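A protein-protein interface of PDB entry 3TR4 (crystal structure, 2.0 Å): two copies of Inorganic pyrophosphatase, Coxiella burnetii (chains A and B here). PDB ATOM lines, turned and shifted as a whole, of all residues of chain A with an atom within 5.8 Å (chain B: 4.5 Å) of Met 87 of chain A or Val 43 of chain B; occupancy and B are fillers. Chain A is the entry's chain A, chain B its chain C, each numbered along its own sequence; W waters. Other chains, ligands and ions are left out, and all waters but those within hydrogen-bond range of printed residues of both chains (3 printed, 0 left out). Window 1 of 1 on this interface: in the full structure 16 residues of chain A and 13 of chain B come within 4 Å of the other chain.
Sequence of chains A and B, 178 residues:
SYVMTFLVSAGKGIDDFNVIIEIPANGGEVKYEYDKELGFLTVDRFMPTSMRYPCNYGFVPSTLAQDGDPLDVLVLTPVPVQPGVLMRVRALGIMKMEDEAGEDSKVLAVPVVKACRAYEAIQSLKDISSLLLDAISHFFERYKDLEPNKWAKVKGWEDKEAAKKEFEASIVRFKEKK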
ATOM      1  N   PHE A  17      -8.091  -2.349 -10.557  1.00  0.00           N
ATOM      2  CA  PHE A  17      -7.994  -1.325  -9.524  1.00  0.00           C
ATOM      3  C   PHE A  17      -8.052   0.094 -10.072  1.00  0.00           C
ATOM      4  O   PHE A  17      -7.894   0.322 -11.273  1.00  0.00           O
ATOM      5  CB  PHE A  17      -6.767  -1.539  -8.619  1.00  0.00           C
ATOM      6  CG  PHE A  17      -5.439  -1.435  -9.327  1.00  0.00           C
ATOM      7  CD1 PHE A  17      -4.694  -0.267  -9.266  1.00  0.00           C
ATOM      8  CD2 PHE A  17      -4.918  -2.518 -10.018  1.00  0.00           C
ATOM      9  CE1 PHE A  17      -3.460  -0.172  -9.897  1.00  0.00           C
ATOM     10  CE2 PHE A  17      -3.687  -2.430 -10.651  1.00  0.00           C
ATOM     11  CZ  PHE A  17      -2.957  -1.253 -10.591  1.00  0.00           C
ATOM     12  N   ASN A  18      -8.298   1.041  -9.176  1.00  0.00           N
ATOM     13  CA  ASN A  18      -8.501   2.431  -9.556  1.00  0.00           C
ATOM     14  C   ASN A  18      -7.221   3.248  -9.555  1.00  0.00           C
ATOM     15  O   ASN A  18      -6.419   3.165  -8.629  1.00  0.00           O
ATOM     16  CB  ASN A  18      -9.518   3.092  -8.628  1.00  0.00           C
ATOM     17  CG  ASN A  18     -10.895   2.484  -8.751  1.00  0.00           C
ATOM     18  OD1 ASN A  18     -11.331   2.125  -9.845  1.00  0.00           O
ATOM     19  ND2 ASN A  18     -11.585   2.358  -7.626  1.00  0.00           N
ATOM     20  N   VAL A  19      -7.039   4.034 -10.609  1.00  0.00           N
ATOM     21  CA  VAL A  19      -5.906   4.937 -10.713  1.00  0.00           C
ATOM     22  C   VAL A  19      -6.404   6.321 -11.088  1.00  0.00           C
ATOM     23  O   VAL A  19      -7.239   6.467 -11.980  1.00  0.00           O
ATOM     24  CB  VAL A  19      -4.901   4.471 -11.784  1.00  0.00           C
ATOM     25  CG1 VAL A  19      -3.798   5.505 -11.967  1.00  0.00           C
ATOM     26  CG2 VAL A  19      -4.312   3.120 -11.404  1.00  0.00           C
ATOM     27  N   ILE A  20      -5.906   7.333 -10.385  1.00  0.00           N
ATOM     28  CA  ILE A  20      -6.156   8.715 -10.752  1.00  0.00           C
ATOM     29  C   ILE A  20      -4.912   9.203 -11.479  1.00  0.00           C
ATOM     30  O   ILE A  20      -3.813   9.183 -10.929  1.00  0.00           O
ATOM     31  CB  ILE A  20      -6.423   9.594  -9.516  1.00  0.00           C
ATOM     32  CG1 ILE A  20      -7.715   9.153  -8.821  1.00  0.00           C
ATOM     33  CG2 ILE A  20      -6.517  11.057  -9.917  1.00  0.00           C
ATOM     34  CD1 ILE A  20      -8.024   9.922  -7.559  1.00  0.00           C
ATOM     35  N   ILE A  21      -5.079   9.608 -12.730  1.00  0.00           N
ATOM     36  CA  ILE A  21      -3.946  10.026 -13.547  1.00  0.00           C
ATOM     37  C   ILE A  21      -3.492  11.438 -13.167  1.00  0.00           C
ATOM     38  O   ILE A  21      -4.312  12.338 -13.012  1.00  0.00           O
ATOM     39  CB  ILE A  21      -4.299   9.973 -15.046  1.00  0.00           C
ATOM     40  CG1 ILE A  21      -4.678   8.546 -15.453  1.00  0.00           C
ATOM     41  CG2 ILE A  21      -3.148  10.492 -15.890  1.00  0.00           C
ATOM     42  CD1 ILE A  21      -3.583   7.514 -15.186  1.00  0.00           C
ATOM     43  N   ASN A  56       1.471   7.154 -19.042  1.00  0.00           N
ATOM     44  CA  ASN A  56       0.688   7.913 -18.077  1.00  0.00           C
ATOM     45  C   ASN A  56       1.143   7.572 -16.666  1.00  0.00           C
ATOM     46  O   ASN A  56       1.589   6.458 -16.399  1.00  0.00           O
ATOM     47  CB  ASN A  56      -0.812   7.647 -18.238  1.00  0.00           C
ATOM     48  CG  ASN A  56      -1.293   7.864 -19.660  1.00  0.00           C
ATOM     49  OD1 ASN A  56      -1.496   8.999 -20.100  1.00  0.00           O
ATOM     50  ND2 ASN A  56      -1.467   6.773 -20.392  1.00  0.00           N
ATOM     51  N   VAL A  75       0.680   3.676 -16.283  1.00  0.00           N
ATOM     52  CA  VAL A  75      -0.368   3.074 -17.104  1.00  0.00           C
ATOM     53  C   VAL A  75      -0.095   3.259 -18.591  1.00  0.00           C
ATOM     54  O   VAL A  75      -0.004   4.384 -19.084  1.00  0.00           O
ATOM     55  CB  VAL A  75      -1.753   3.639 -16.753  1.00  0.00           C
ATOM     56  CG1 VAL A  75      -2.842   2.884 -17.514  1.00  0.00           C
ATOM     57  CG2 VAL A  75      -1.988   3.551 -15.246  1.00  0.00           C
ATOM     58  N   THR A  77      -1.287   3.159 -22.339  1.00  0.00           N
ATOM     59  CA  THR A  77      -2.545   3.335 -23.061  1.00  0.00           C
ATOM     60  C   THR A  77      -2.265   3.634 -24.531  1.00  0.00           C
ATOM     61  O   THR A  77      -1.178   4.098 -24.869  1.00  0.00           O
ATOM     62  CB  THR A  77      -3.359   4.503 -22.472  1.00  0.00           C
ATOM     63  OG1 THR A  77      -2.600   5.717 -22.579  1.00  0.00           O
ATOM     64  CG2 THR A  77      -3.681   4.239 -21.008  1.00  0.00           C
ATOM     65  N   VAL A  81      -3.928  10.018 -21.541  1.00  0.00           N
ATOM     66  CA  VAL A  81      -5.146  10.241 -20.784  1.00  0.00           C
ATOM     67  C   VAL A  81      -5.081  11.610 -20.109  1.00  0.00           C
ATOM     68  O   VAL A  81      -4.035  12.006 -19.599  1.00  0.00           O
ATOM     69  CB  VAL A  81      -5.331   9.129 -19.739  1.00  0.00           C
ATOM     70  CG1 VAL A  81      -6.365   9.514 -18.718  1.00  0.00           C
ATOM     71  CG2 VAL A  81      -5.715   7.826 -20.433  1.00  0.00           C
ATOM     72  N   VAL A  85      -8.205  12.378 -14.430  1.00  0.00           N
ATOM     73  CA  VAL A  85      -9.166  11.330 -14.769  1.00  0.00           C
ATOM     74  C   VAL A  85      -8.932  10.047 -13.970  1.00  0.00           C
ATOM     75  O   VAL A  85      -7.787   9.663 -13.716  1.00  0.00           O
ATOM     76  CB  VAL A  85      -9.091  10.983 -16.279  1.00  0.00           C
ATOM     77  CG1 VAL A  85      -9.930   9.752 -16.598  1.00  0.00           C
ATOM     78  CG2 VAL A  85      -9.533  12.169 -17.125  1.00  0.00           C
ATOM     79  N   LEU A  86     -10.020   9.383 -13.581  1.00  0.00           N
ATOM     80  CA  LEU A  86      -9.921   8.100 -12.898  1.00  0.00           C
ATOM     81  C   LEU A  86     -10.116   6.991 -13.921  1.00  0.00           C
ATOM     82  O   LEU A  86     -10.961   7.103 -14.806  1.00  0.00           O
ATOM     83  CB  LEU A  86     -11.006   8.022 -11.817  1.00  0.00           C
ATOM     84  CG  LEU A  86     -11.223   6.749 -10.988  1.00  0.00           C
ATOM     85  CD1 LEU A  86     -12.002   5.686 -11.762  1.00  0.00           C
ATOM     86  CD2 LEU A  86      -9.907   6.200 -10.468  1.00  0.00           C
ATOM     87  N   MET A  87      -9.339   5.922 -13.812  1.00  0.00           N
ATOM     88  CA  MET A  87      -9.508   4.793 -14.718  1.00  0.00           C
ATOM     89  C   MET A  87      -9.283   3.458 -14.023  1.00  0.00           C
ATOM     90  O   MET A  87      -8.627   3.385 -12.984  1.00  0.00           O
ATOM     91  CB  MET A  87      -8.604   4.935 -15.948  1.00  0.00           C
ATOM     92  CG  MET A  87      -7.116   4.925 -15.642  1.00  0.00           C
ATOM     93  SD  MET A  87      -6.024   5.403 -17.197  1.00  0.00           S
ATOM     94  CE  MET A  87      -6.628   4.007 -18.425  1.00  0.00           C
ATOM     95  N   ARG A  88      -9.853   2.405 -14.595  1.00  0.00           N
ATOM     96  CA  ARG A  88      -9.713   1.070 -14.038  1.00  0.00           C
ATOM     97  C   ARG A  88      -8.655   0.304 -14.809  1.00  0.00           C
ATOM     98  O   ARG A  88      -8.722   0.206 -16.035  1.00  0.00           O
ATOM     99  CB  ARG A  88     -11.054   0.333 -14.075  1.00  0.00           C
ATOM    100  CG  ARG A  88     -12.079   0.906 -13.109  1.00  0.00           C
ATOM    101  CD  ARG A  88     -13.470   0.350 -13.353  1.00  0.00           C
ATOM    102  NE  ARG A  88     -13.523  -1.105 -13.238  1.00  0.00           N
ATOM    103  CZ  ARG A  88     -14.654  -1.797 -13.141  1.00  0.00           C
ATOM    104  NH1 ARG A  88     -15.819  -1.161 -13.137  1.00  0.00           N
ATOM    105  NH2 ARG A  88     -14.626  -3.119 -13.039  1.00  0.00           N
ATOM    106  N   VAL A  89      -7.673  -0.230 -14.086  1.00  0.00           N
ATOM    107  CA  VAL A  89      -6.524  -0.876 -14.714  1.00  0.00           C
ATOM    108  C   VAL A  89      -6.191  -2.232 -14.100  1.00  0.00           C
ATOM    109  O   VAL A  89      -6.715  -2.609 -13.049  1.00  0.00           O
ATOM    110  CB  VAL A  89      -5.264   0.002 -14.623  1.00  0.00           C
ATOM    111  CG1 VAL A  89      -5.514   1.368 -15.249  1.00  0.00           C
ATOM    112  CG2 VAL A  89      -4.825   0.146 -13.174  1.00  0.00           C
ATOM    113  N   PRO A 111      -5.122  -0.777 -19.174  1.00  0.00           N
ATOM    114  CA  PRO A 111      -6.561  -0.720 -18.881  1.00  0.00           C
ATOM    115  C   PRO A 111      -7.198  -2.104 -18.750  1.00  0.00           C
ATOM    116  O   PRO A 111      -6.709  -3.066 -19.348  1.00  0.00           O
ATOM    117  CB  PRO A 111      -7.139  -0.005 -20.108  1.00  0.00           C
ATOM    118  CG  PRO A 111      -6.010   0.793 -20.655  1.00  0.00           C
ATOM    119  CD  PRO A 111      -4.771  -0.021 -20.389  1.00  0.00           C
ATOM    120  N   LYS A 114     -12.333  -4.404 -20.759  1.00  0.00           N
ATOM    121  CA  LYS A 114     -13.500  -3.657 -21.216  1.00  0.00           C
ATOM    122  C   LYS A 114     -13.102  -2.309 -21.811  1.00  0.00           C
ATOM    123  O   LYS A 114     -13.698  -1.849 -22.791  1.00  0.00           O
ATOM    124  CB  LYS A 114     -14.490  -3.466 -20.062  1.00  0.00           C
ATOM    125  CG  LYS A 114     -15.575  -2.433 -20.311  1.00  0.00           C
ATOM    126  CD  LYS A 114     -15.268  -1.125 -19.597  1.00  0.00           C
ATOM    127  CE  LYS A 114     -16.412  -0.133 -19.749  1.00  0.00           C
ATOM    128  NZ  LYS A 114     -16.142   1.154 -19.046  1.00  0.00           N
ATOM    129  N   ALA A 115     -12.083  -1.686 -21.226  1.00  0.00           N
ATOM    130  CA  ALA A 115     -11.659  -0.354 -21.645  1.00  0.00           C
ATOM    131  C   ALA A 115     -10.706  -0.379 -22.839  1.00  0.00           C
ATOM    132  O   ALA A 115     -10.613   0.592 -23.584  1.00  0.00           O
ATOM    133  CB  ALA A 115     -11.024   0.389 -20.475  1.00  0.00           C
ATOM    134  N   VAL B  30      -9.978   8.154 -27.105  1.00  0.00           N
ATOM    135  CA  VAL B  30     -10.336   7.761 -25.752  1.00  0.00           C
ATOM    136  C   VAL B  30     -11.708   8.337 -25.422  1.00  0.00           C
ATOM    137  O   VAL B  30     -11.934   9.536 -25.554  1.00  0.00           O
ATOM    138  CB  VAL B  30      -9.304   8.250 -24.708  1.00  0.00           C
ATOM    139  CG1 VAL B  30      -9.095   9.752 -24.815  1.00  0.00           C
ATOM    140  CG2 VAL B  30      -9.753   7.867 -23.306  1.00  0.00           C
ATOM    141  N   LYS B  31     -12.630   7.469 -25.020  1.00  0.00           N
ATOM    142  CA  LYS B  31     -13.958   7.886 -24.593  1.00  0.00           C
ATOM    143  C   LYS B  31     -13.959   8.079 -23.092  1.00  0.00           C
ATOM    144  O   LYS B  31     -13.647   7.150 -22.351  1.00  0.00           O
ATOM    145  CB  LYS B  31     -14.988   6.805 -24.920  1.00  0.00           C
ATOM    146  CG  LYS B  31     -15.826   7.067 -26.143  1.00  0.00           C
ATOM    147  CD  LYS B  31     -14.994   6.958 -27.396  1.00  0.00           C
ATOM    148  CE  LYS B  31     -15.876   6.880 -28.631  1.00  0.00           C
ATOM    149  NZ  LYS B  31     -15.072   6.730 -29.880  1.00  0.00           N
ATOM    150  N   TYR B  32     -14.316   9.275 -22.643  1.00  0.00           N
ATOM    151  CA  TYR B  32     -14.510   9.514 -21.220  1.00  0.00           C
ATOM    152  C   TYR B  32     -15.993   9.422 -20.896  1.00  0.00           C
ATOM    153  O   TYR B  32     -16.833   9.569 -21.778  1.00  0.00           O
ATOM    154  CB  TYR B  32     -13.983  10.896 -20.823  1.00  0.00           C
ATOM    155  CG  TYR B  32     -12.502  11.085 -21.090  1.00  0.00           C
ATOM    156  CD1 TYR B  32     -11.550  10.479 -20.282  1.00  0.00           C
ATOM    157  CD2 TYR B  32     -12.059  11.867 -22.149  1.00  0.00           C
ATOM    158  CE1 TYR B  32     -10.201  10.644 -20.518  1.00  0.00           C
ATOM    159  CE2 TYR B  32     -10.701  12.041 -22.394  1.00  0.00           C
ATOM    160  CZ  TYR B  32      -9.783  11.424 -21.573  1.00  0.00           C
ATOM    161  OH  TYR B  32      -8.437  11.587 -21.804  1.00  0.00           O
ATOM    162  N   THR B  42     -14.103   9.742 -15.853  1.00  0.00           N
ATOM    163  CA  THR B  42     -13.428   8.452 -15.924  1.00  0.00           C
ATOM    164  C   THR B  42     -13.194   8.036 -17.363  1.00  0.00           C
ATOM    165  O   THR B  42     -13.804   8.578 -18.281  1.00  0.00           O
ATOM    166  CB  THR B  42     -14.251   7.342 -15.244  1.00  0.00           C
ATOM    167  OG1 THR B  42     -15.451   7.112 -15.995  1.00  0.00           O
ATOM    168  CG2 THR B  42     -14.609   7.734 -13.819  1.00  0.00           C
ATOM    169  N   VAL B  43     -12.299   7.075 -17.555  1.00  0.00           N
ATOM    170  CA  VAL B  43     -12.134   6.457 -18.859  1.00  0.00           C
ATOM    171  C   VAL B  43     -13.243   5.442 -19.084  1.00  0.00           C
ATOM    172  O   VAL B  43     -13.473   4.563 -18.254  1.00  0.00           O
ATOM    173  CB  VAL B  43     -10.785   5.732 -18.994  1.00  0.00           C
ATOM    174  CG1 VAL B  43     -10.830   4.761 -20.166  1.00  0.00           C
ATOM    175  CG2 VAL B  43      -9.647   6.733 -19.153  1.00  0.00           C
ATOM    176  N   ASP B  44     -13.933   5.575 -20.210  1.00  0.00           N
ATOM    177  CA  ASP B  44     -14.933   4.607 -20.624  1.00  0.00           C
ATOM    178  C   ASP B  44     -14.240   3.505 -21.409  1.00  0.00           C
ATOM    179  O   ASP B  44     -14.127   2.370 -20.947  1.00  0.00           O
ATOM    180  CB  ASP B  44     -15.978   5.287 -21.510  1.00  0.00           C
ATOM    181  CG  ASP B  44     -17.058   4.334 -21.991  1.00  0.00           C
ATOM    182  OD1 ASP B  44     -16.967   3.119 -21.711  1.00  0.00           O
ATOM    183  OD2 ASP B  44     -18.000   4.803 -22.662  1.00  0.00           O
ATOM    184  N   ARG B  45     -13.772   3.856 -22.602  1.00  0.00           N
ATOM    185  CA  ARG B  45     -13.094   2.918 -23.483  1.00  0.00           C
ATOM    186  C   ARG B  45     -12.158   3.656 -24.426  1.00  0.00           C
ATOM    187  O   ARG B  45     -12.360   4.829 -24.727  1.00  0.00           O
ATOM    188  CB  ARG B  45     -14.105   2.140 -24.329  1.00  0.00           C
ATOM    189  CG  ARG B  45     -15.093   1.300 -23.552  1.00  0.00           C
ATOM    190  CD  ARG B  45     -16.021   0.560 -24.496  1.00  0.00           C
ATOM    191  NE  ARG B  45     -17.166  -0.012 -23.795  1.00  0.00           N
ATOM    192  CZ  ARG B  45     -18.293   0.649 -23.550  1.00  0.00           C
ATOM    193  NH1 ARG B  45     -18.425   1.907 -23.951  1.00  0.00           N
ATOM    194  NH2 ARG B  45     -19.288   0.055 -22.905  1.00  0.00           N
ATOM    195  N   PHE B  46     -11.139   2.950 -24.895  1.00  0.00           N
ATOM    196  CA  PHE B  46     -10.308   3.424 -25.992  1.00  0.00           C
ATOM    197  C   PHE B  46     -10.834   2.812 -27.282  1.00  0.00           C
ATOM    198  O   PHE B  46     -11.135   1.619 -27.338  1.00  0.00           O
ATOM    199  CB  PHE B  46      -8.847   3.026 -25.773  1.00  0.00           C
ATOM    200  CG  PHE B  46      -8.220   3.673 -24.570  1.00  0.00           C
ATOM    201  CD1 PHE B  46      -7.580   4.899 -24.680  1.00  0.00           C
ATOM    202  CD2 PHE B  46      -8.275   3.062 -23.329  1.00  0.00           C
ATOM    203  CE1 PHE B  46      -7.007   5.500 -23.576  1.00  0.00           C
ATOM    204  CE2 PHE B  46      -7.699   3.660 -22.220  1.00  0.00           C
ATOM    205  CZ  PHE B  46      -7.068   4.879 -22.344  1.00  0.00           C
HETATM  206  O   HOH W   1     -16.133   3.741 -16.721  1.00  0.00           O
HETATM  207  O   HOH W   2     -12.208   2.879 -16.549  1.00  0.00           O
HETATM  208  O   HOH W   3     -11.668  -0.958 -26.213  1.00  0.00           O
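No position is printed for both chains. Of the 16 pairs that touch across the chains among the printed residues, none has its exchanged pair printed and touching as well.
Hydrophobic or aromatic side chains of chain B within 4 Å of the printed part of chain A: Tyr 32, Val 43 and Phe 46. Of the 17 printed residues of chain A, 8 touch a printed residue of chain B. Printed residues of chain A that touch a printed residue of chain B: Thr 77, Val 81, Val 85, Leu 86, Met 87, Pro 111, Lys 114 and Ala 115. Hydrophobic or aromatic side chains of chain A within 4 Å of the printed part of chain B: Val 81, Val 85, Leu 86, Met 87, Pro 111 and Ala 115. Among the printed residues, 16 pairs touch across the chains. Among the printed residues, Asp or Glu carboxylates within 4 Å of a Lys or Arg side-chain nitrogen of the other chain: Lys 114 of chain A with Asp 44 of chain B (3.4 Å).
Among the printed residues, merely in contact across the chains: Thr 77 of chain A with Phe 46 of chain B, Val 81 of chain A with Tyr 32 of chain B, Val 81 of chain A with Phe 46 of chain B, Val 85 of chain A with Tyr 32 of chain B, Val 85 of chain A with Thr 42 of chain B, Val 85 of chain A with Val 43 of chain B, Leu 86 of chain A with Thr 42 of chain B, Met 87 of chain A with Val 43 of chain B, Met 87 of chain A with Phe 46 of chain B, Pro 111 of chain A with Phe 46 of chain B, Lys 114 of chain A with Arg 45 of chain B, Ala 115 of chain A with Asp 44 of chain B and Ala 115 of chain A with Arg 45 of chain B.
The side-chain amino group of Lys 114 of chain A lies within salt-bridge range of the side-chain carboxylate of Asp 44 of chain B, 3.4 Å away. The backbone NH of Phe 46 of chain B sits at hydrogen-bond distance from the backbone carbonyl oxygen of Ala 115 of chain A. The backbone NH of Val 43 of chain B sits at hydrogen-bond distance from the backbone carbonyl oxygen of Leu 86 of chain A (3.1 Å).
Water W2 lies within hydrogen-bond range of the backbone carbonyl oxygen (O) of Val 43 of chain B and the backbone NH (N) of Arg 88 of chain A. Water W3 bridges the backbone carbonyl oxygen (O) of Phe 46 of chain B (2.9 Å) and the backbone carbonyl oxygen (O) of Ala 115 of chain A (3.2 Å). Water W1 bridges O of Val 43 of chain B (3.2 Å) and NZ of Lys 114 of chain A (3.5 Å).
Of the printed residues of chain A, Asp 44 of chain B touches Lys 114 and Ala 115. Printed residues of chain A within 4 Å of Tyr 32 of chain B: Val 81 (3.7 Å) and Val 85 (3.8 Å). Printed residues of chain B within 4 Å of Val 85 of chain A: Tyr 32, Thr 42 and Val 43. Printed residues of chain B within 4 Å of Ala 115 of chain A: Asp 44 (3.7 Å), Arg 45 (3.4 Å) and Phe 46 (2.7 Å). Ile 21 of chain A touches none of the printed residues of chain B.
N of Lys 31 of chain B is in hydrogen-bond range of O of Arg 45 of chain B. The backbone carbonyl oxygen of Val 19 of chain A is in hydrogen-bond range of the backbone NH of Met 87 of chain A (2.8 Å). N of Val 81 of chain A sits at hydrogen-bond distance from OD1 of Asn 56 of chain A (3.0 Å). The backbone NH (N) of Ile 21 of chain A is in hydrogen-bond range of the backbone carbonyl oxygen (O) of Val 85 of chain A (2.9 Å). The guanidinium group (NH1) of Arg 45 of chain B is in salt-bridge range of the side-chain carboxylate (OD1) of Asp 44 of chain B, 2.9 Å away. The backbone carbonyl oxygen (O) of Lys 31 of chain B lies within hydrogen-bond range of the backbone NH (N) of Asp 44 of chain B (2.7 Å).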
